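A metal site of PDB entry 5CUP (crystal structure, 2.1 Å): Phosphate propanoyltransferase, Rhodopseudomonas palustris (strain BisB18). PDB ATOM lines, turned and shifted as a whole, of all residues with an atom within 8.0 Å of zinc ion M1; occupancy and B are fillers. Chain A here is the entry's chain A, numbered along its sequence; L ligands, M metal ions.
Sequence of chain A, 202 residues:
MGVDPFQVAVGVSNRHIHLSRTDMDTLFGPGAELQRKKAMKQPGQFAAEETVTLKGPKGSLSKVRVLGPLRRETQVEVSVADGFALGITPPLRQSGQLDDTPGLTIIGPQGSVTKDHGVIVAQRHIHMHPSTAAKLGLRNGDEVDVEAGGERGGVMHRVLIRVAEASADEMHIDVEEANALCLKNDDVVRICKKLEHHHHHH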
ATOM      1  N   SER A  13     -17.291  34.318   3.633  1.00  0.00           N
ATOM      2  CA  SER A  13     -15.955  33.822   3.933  1.00  0.00           C
ATOM      3  C   SER A  13     -15.221  33.349   2.680  1.00  0.00           C
ATOM      4  O   SER A  13     -15.542  32.315   2.107  1.00  0.00           O
ATOM      5  CB  SER A  13     -16.034  32.688   4.940  1.00  0.00           C
ATOM      6  OG  SER A  13     -14.943  31.797   4.791  1.00  0.00           O
ATOM      7  N   ASN A  14     -14.223  34.131   2.270  1.00  0.00           N
ATOM      8  CA  ASN A  14     -13.350  33.718   1.178  1.00  0.00           C
ATOM      9  C   ASN A  14     -12.430  32.606   1.667  1.00  0.00           C
ATOM     10  O   ASN A  14     -12.355  32.347   2.863  1.00  0.00           O
ATOM     11  CB  ASN A  14     -12.541  34.916   0.674  1.00  0.00           C
ATOM     12  CG  ASN A  14     -11.849  34.640  -0.651  1.00  0.00           C
ATOM     13  OD1 ASN A  14     -12.066  33.608  -1.275  1.00  0.00           O
ATOM     14  ND2 ASN A  14     -11.022  35.584  -1.084  1.00  0.00           N
ATOM     15  N   ARG A  15     -11.746  31.947   0.742  1.00  0.00           N
ATOM     16  CA  ARG A  15     -10.800  30.899   1.103  1.00  0.00           C
ATOM     17  C   ARG A  15      -9.796  31.430   2.120  1.00  0.00           C
ATOM     18  O   ARG A  15      -9.366  32.572   2.035  1.00  0.00           O
ATOM     19  CB  ARG A  15     -10.059  30.371  -0.131  1.00  0.00           C
ATOM     20  CG  ARG A  15      -9.034  31.354  -0.693  1.00  0.00           C
ATOM     21  CD  ARG A  15      -8.363  30.791  -1.931  1.00  0.00           C
ATOM     22  NE  ARG A  15      -9.279  30.713  -3.069  1.00  0.00           N
ATOM     23  CZ  ARG A  15      -9.161  31.408  -4.205  1.00  0.00           C
ATOM     24  NH1 ARG A  15     -10.061  31.243  -5.161  1.00  0.00           N
ATOM     25  NH2 ARG A  15      -8.153  32.252  -4.400  1.00  0.00           N
ATOM     26  N   HIS A  16      -9.453  30.599   3.096  1.00  0.00           N
ATOM     27  CA  HIS A  16      -8.522  31.006   4.143  1.00  0.00           C
ATOM     28  C   HIS A  16      -7.949  29.816   4.894  1.00  0.00           C
ATOM     29  O   HIS A  16      -8.309  28.662   4.625  1.00  0.00           O
ATOM     30  CB  HIS A  16      -9.214  31.951   5.127  1.00  0.00           C
ATOM     31  CG  HIS A  16     -10.343  31.325   5.876  1.00  0.00           C
ATOM     32  ND1 HIS A  16     -11.664  31.435   5.483  1.00  0.00           N
ATOM     33  CD2 HIS A  16     -10.354  30.578   7.008  1.00  0.00           C
ATOM     34  CE1 HIS A  16     -12.425  30.782   6.336  1.00  0.00           C
ATOM     35  NE2 HIS A  16     -11.658  30.253   7.269  1.00  0.00           N
ATOM     36  N   ILE A  17      -7.057  30.098   5.833  1.00  0.00           N
ATOM     37  CA  ILE A  17      -6.360  29.055   6.562  1.00  0.00           C
ATOM     38  C   ILE A  17      -6.172  29.425   8.027  1.00  0.00           C
ATOM     39  O   ILE A  17      -5.920  30.577   8.361  1.00  0.00           O
ATOM     40  CB  ILE A  17      -4.977  28.758   5.926  1.00  0.00           C
ATOM     41  CG1 ILE A  17      -4.313  27.579   6.636  1.00  0.00           C
ATOM     42  CG2 ILE A  17      -4.083  30.000   5.977  1.00  0.00           C
ATOM     43  CD1 ILE A  17      -3.090  27.046   5.904  1.00  0.00           C
ATOM     44  N   HIS A  18      -6.334  28.423   8.893  1.00  0.00           N
ATOM     45  CA  HIS A  18      -5.973  28.548  10.308  1.00  0.00           C
ATOM     46  C   HIS A  18      -4.689  27.749  10.524  1.00  0.00           C
ATOM     47  O   HIS A  18      -4.546  26.660   9.982  1.00  0.00           O
ATOM     48  CB  HIS A  18      -7.094  28.041  11.202  1.00  0.00           C
ATOM     49  CG  HIS A  18      -8.442  28.610  10.881  1.00  0.00           C
ATOM     50  ND1 HIS A  18      -8.912  29.773  11.439  1.00  0.00           N
ATOM     51  CD2 HIS A  18      -9.408  28.175  10.031  1.00  0.00           C
ATOM     52  CE1 HIS A  18     -10.120  30.029  10.957  1.00  0.00           C
ATOM     53  NE2 HIS A  18     -10.444  29.080  10.111  1.00  0.00           N
ATOM     54  N   MET A  40     -12.423  40.961  12.618  1.00  0.00           N
ATOM     55  CA  MET A  40     -13.650  40.327  12.149  1.00  0.00           C
ATOM     56  C   MET A  40     -14.770  40.503  13.164  1.00  0.00           C
ATOM     57  O   MET A  40     -14.552  41.016  14.257  1.00  0.00           O
ATOM     58  CB  MET A  40     -13.401  38.831  11.880  1.00  0.00           C
ATOM     59  CG  MET A  40     -12.651  38.561  10.588  1.00  0.00           C
ATOM     60  SD  MET A  40     -11.936  36.910  10.509  1.00  0.00           S
ATOM     61  CE  MET A  40     -13.318  35.902  11.060  1.00  0.00           C
ATOM     62  N   GLN A  45     -11.129  37.248  16.680  1.00  0.00           N
ATOM     63  CA  GLN A  45     -10.698  36.763  15.383  1.00  0.00           C
ATOM     64  C   GLN A  45     -10.452  37.921  14.422  1.00  0.00           C
ATOM     65  O   GLN A  45     -11.065  38.975  14.547  1.00  0.00           O
ATOM     66  CB  GLN A  45     -11.741  35.807  14.798  1.00  0.00           C
ATOM     67  CG  GLN A  45     -12.013  34.600  15.678  1.00  0.00           C
ATOM     68  CD  GLN A  45     -12.422  33.373  14.884  1.00  0.00           C
ATOM     69  OE1 GLN A  45     -11.715  32.944  13.977  1.00  0.00           O
ATOM     70  NE2 GLN A  45     -13.570  32.805  15.235  1.00  0.00           N
ATOM     71  N   LEU A  67      -6.093  33.566   8.928  1.00  0.00           N
ATOM     72  CA  LEU A  67      -6.922  34.135   9.982  1.00  0.00           C
ATOM     73  C   LEU A  67      -6.328  33.859  11.354  1.00  0.00           C
ATOM     74  O   LEU A  67      -5.943  32.727  11.659  1.00  0.00           O
ATOM     75  CB  LEU A  67      -8.346  33.563   9.917  1.00  0.00           C
ATOM     76  CG  LEU A  67      -9.176  33.840   8.664  1.00  0.00           C
ATOM     77  CD1 LEU A  67     -10.589  33.290   8.867  1.00  0.00           C
ATOM     78  CD2 LEU A  67      -9.235  35.319   8.336  1.00  0.00           C
ATOM     79  N   ARG A  71      -4.349  28.453  16.166  1.00  0.00           N
ATOM     80  CA  ARG A  71      -5.174  27.409  16.758  1.00  0.00           C
ATOM     81  C   ARG A  71      -4.340  26.173  17.079  1.00  0.00           C
ATOM     82  O   ARG A  71      -3.135  26.159  16.851  1.00  0.00           O
ATOM     83  CB  ARG A  71      -6.341  27.051  15.827  1.00  0.00           C
ATOM     84  CG  ARG A  71      -7.364  28.163  15.678  1.00  0.00           C
ATOM     85  CD  ARG A  71      -8.535  27.729  14.824  1.00  0.00           C
ATOM     86  NE  ARG A  71      -9.552  28.772  14.703  1.00  0.00           N
ATOM     87  CZ  ARG A  71     -10.631  28.697  13.936  1.00  0.00           C
ATOM     88  NH1 ARG A  71     -10.848  27.612  13.193  1.00  0.00           N
ATOM     89  NH2 ARG A  71     -11.489  29.705  13.900  1.00  0.00           N
ATOM     90  N   GLN A  75      -6.062  24.147   9.647  1.00  0.00           N
ATOM     91  CA  GLN A  75      -7.282  23.876   8.901  1.00  0.00           C
ATOM     92  C   GLN A  75      -7.402  24.810   7.702  1.00  0.00           C
ATOM     93  O   GLN A  75      -7.312  26.032   7.847  1.00  0.00           O
ATOM     94  CB  GLN A  75      -8.516  24.031   9.808  1.00  0.00           C
ATOM     95  CG  GLN A  75      -9.857  23.871   9.089  1.00  0.00           C
ATOM     96  CD  GLN A  75     -11.045  24.015  10.028  1.00  0.00           C
ATOM     97  OE1 GLN A  75     -11.309  23.141  10.858  1.00  0.00           O
ATOM     98  NE2 GLN A  75     -11.761  25.125   9.905  1.00  0.00           N
ATOM     99  N   VAL A  76      -7.592  24.222   6.526  1.00  0.00           N
ATOM    100  CA  VAL A  76      -7.765  24.975   5.285  1.00  0.00           C
ATOM    101  C   VAL A  76      -9.207  24.894   4.808  1.00  0.00           C
ATOM    102  O   VAL A  76      -9.780  23.805   4.723  1.00  0.00           O
ATOM    103  CB  VAL A  76      -6.843  24.454   4.181  1.00  0.00           C
ATOM    104  CG1 VAL A  76      -6.848  25.416   2.995  1.00  0.00           C
ATOM    105  CG2 VAL A  76      -5.424  24.277   4.700  1.00  0.00           C
ATOM    106  N   GLU A  77      -9.783  26.041   4.486  1.00  0.00           N
ATOM    107  CA  GLU A  77     -11.144  26.115   3.964  1.00  0.00           C
ATOM    108  C   GLU A  77     -11.150  26.673   2.552  1.00  0.00           C
ATOM    109  O   GLU A  77     -10.750  27.811   2.324  1.00  0.00           O
ATOM    110  CB  GLU A  77     -12.020  26.963   4.888  1.00  0.00           C
ATOM    111  CG  GLU A  77     -12.312  26.292   6.219  1.00  0.00           C
ATOM    112  CD  GLU A  77     -12.831  27.268   7.250  1.00  0.00           C
ATOM    113  OE1 GLU A  77     -12.187  27.401   8.309  1.00  0.00           O
ATOM    114  OE2 GLU A  77     -13.895  27.884   7.011  1.00  0.00           O
ATOM    115  N   SER A  95     -16.337  23.169  11.032  1.00  0.00           N
ATOM    116  CA  SER A  95     -15.018  23.458  11.579  1.00  0.00           C
ATOM    117  C   SER A  95     -14.592  22.425  12.629  1.00  0.00           C
ATOM    118  O   SER A  95     -15.368  22.078  13.517  1.00  0.00           O
ATOM    119  CB  SER A  95     -14.996  24.855  12.197  1.00  0.00           C
ATOM    120  OG  SER A  95     -14.188  25.738  11.446  1.00  0.00           O
ATOM    121  N   ILE A 120     -11.043  21.267   3.948  1.00  0.00           N
ATOM    122  CA  ILE A 120     -12.483  21.020   3.830  1.00  0.00           C
ATOM    123  C   ILE A 120     -13.178  22.106   3.011  1.00  0.00           C
ATOM    124  O   ILE A 120     -12.650  23.199   2.819  1.00  0.00           O
ATOM    125  CB  ILE A 120     -13.150  20.951   5.219  1.00  0.00           C
ATOM    126  CG1 ILE A 120     -12.929  22.253   5.985  1.00  0.00           C
ATOM    127  CG2 ILE A 120     -12.596  19.759   6.002  1.00  0.00           C
ATOM    128  CD1 ILE A 120     -13.821  22.408   7.213  1.00  0.00           C
ATOM    129  N   ALA A 122     -16.259  24.349   3.677  1.00  0.00           N
ATOM    130  CA  ALA A 122     -16.982  24.780   4.870  1.00  0.00           C
ATOM    131  C   ALA A 122     -18.485  24.582   4.721  1.00  0.00           C
ATOM    132  O   ALA A 122     -19.101  25.065   3.764  1.00  0.00           O
ATOM    133  CB  ALA A 122     -16.668  26.225   5.182  1.00  0.00           C
ATOM    134  N   HIS A 125     -23.048  27.911   8.263  1.00  0.00           N
ATOM    135  CA  HIS A 125     -23.362  27.881   9.684  1.00  0.00           C
ATOM    136  C   HIS A 125     -23.653  29.275  10.219  1.00  0.00           C
ATOM    137  O   HIS A 125     -23.378  30.278   9.549  1.00  0.00           O
ATOM    138  CB  HIS A 125     -22.206  27.255  10.462  1.00  0.00           C
ATOM    139  CG  HIS A 125     -20.898  27.968  10.263  1.00  0.00           C
ATOM    140  ND1 HIS A 125     -20.048  27.694   9.208  1.00  0.00           N
ATOM    141  CD2 HIS A 125     -20.296  28.936  10.990  1.00  0.00           C
ATOM    142  CE1 HIS A 125     -18.984  28.463   9.289  1.00  0.00           C
ATOM    143  NE2 HIS A 125     -19.107  29.225  10.362  1.00  0.00           N
ATOM    144  N   HIS A 127     -22.864  31.506  13.673  1.00  0.00           N
ATOM    145  CA  HIS A 127     -22.303  31.751  15.004  1.00  0.00           C
ATOM    146  C   HIS A 127     -23.333  32.509  15.810  1.00  0.00           C
ATOM    147  O   HIS A 127     -23.813  33.558  15.383  1.00  0.00           O
ATOM    148  CB  HIS A 127     -21.003  32.549  14.906  1.00  0.00           C
ATOM    149  CG  HIS A 127     -19.920  31.873  14.134  1.00  0.00           C
ATOM    150  ND1 HIS A 127     -19.137  30.869  14.668  1.00  0.00           N
ATOM    151  CD2 HIS A 127     -19.471  32.066  12.873  1.00  0.00           C
ATOM    152  CE1 HIS A 127     -18.276  30.464  13.754  1.00  0.00           C
ATOM    153  NE2 HIS A 127     -18.444  31.177  12.661  1.00  0.00           N
ATOM    154  N   ARG A 162     -24.120  27.183  15.584  1.00  0.00           N
ATOM    155  CA  ARG A 162     -22.913  27.123  16.407  1.00  0.00           C
ATOM    156  C   ARG A 162     -22.996  28.122  17.552  1.00  0.00           C
ATOM    157  O   ARG A 162     -22.841  29.337  17.349  1.00  0.00           O
ATOM    158  CB  ARG A 162     -21.675  27.405  15.558  1.00  0.00           C
ATOM    159  CG  ARG A 162     -20.947  26.159  15.086  1.00  0.00           C
ATOM    160  CD  ARG A 162     -19.538  26.463  14.595  1.00  0.00           C
ATOM    161  NE  ARG A 162     -18.753  27.178  15.599  1.00  0.00           N
ATOM    162  CZ  ARG A 162     -17.437  27.341  15.562  1.00  0.00           C
ATOM    163  NH1 ARG A 162     -16.725  26.828  14.567  1.00  0.00           N
ATOM    164  NH2 ARG A 162     -16.820  28.008  16.521  1.00  0.00           N
ATOM    165  N   HIS A 172     -22.058  32.478   8.255  1.00  0.00           N
ATOM    166  CA  HIS A 172     -20.893  32.294   7.394  1.00  0.00           C
ATOM    167  C   HIS A 172     -21.203  31.373   6.216  1.00  0.00           C
ATOM    168  O   HIS A 172     -21.632  30.233   6.410  1.00  0.00           O
ATOM    169  CB  HIS A 172     -19.710  31.747   8.194  1.00  0.00           C
ATOM    170  CG  HIS A 172     -18.979  32.789   8.985  1.00  0.00           C
ATOM    171  ND1 HIS A 172     -18.119  32.470  10.023  1.00  0.00           N
ATOM    172  CD2 HIS A 172     -18.949  34.136   8.879  1.00  0.00           C
ATOM    173  CE1 HIS A 172     -17.605  33.581  10.520  1.00  0.00           C
ATOM    174  NE2 HIS A 172     -18.095  34.606   9.848  1.00  0.00           N
HETATM  175  P1  LIG L   1     -14.437  29.417  11.164  1.00  0.00           P
HETATM  176  O1  LIG L   1     -13.673  29.947  12.350  1.00  0.00           O
HETATM  177  O2  LIG L   1     -13.894  30.024   9.895  1.00  0.00           O
HETATM  178  O3  LIG L   1     -15.899  29.772  11.311  1.00  0.00           O
HETATM  179  O4  LIG L   1     -14.308  27.917  11.110  1.00  0.00           O
HETATM  180 ZN    ZN M   1     -12.224  29.242   9.009  1.00  0.00          ZN
HETATM  181 ZN    ZN M   2     -17.557  30.716  10.795  1.00  0.00          ZN
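The side-chain carboxylate (OE1) of Glu 77 lies close to the side-chain amide nitrogen (NE2) of Gln 75, 2.8 Å away. ND1 of His 16 lies close to OG of Ser 13, at 3.4 Å. A ring nitrogen (ND1) of His 16 sits at hydrogen-bond distance from the backbone carbonyl oxygen (O) of Asn 14. The backbone NH (N) of His 18 lies within hydrogen-bond range of the backbone carbonyl oxygen (O) of Gln 75. A ring nitrogen (ND1) of His 18 lies close to the guanidinium group (NH1) of Arg 71 (3.4 Å).
Of the 20 residues printed, 3 come within 4 Å of zinc ion M1. The nearest printed residue that does not touch zinc ion M1 is Gln 75 (4.2 Å).
Zinc ion M1 is bound by OE1 of Glu 77, O2 of the ligand, NE2 of His 16 and NE2 of His 18.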
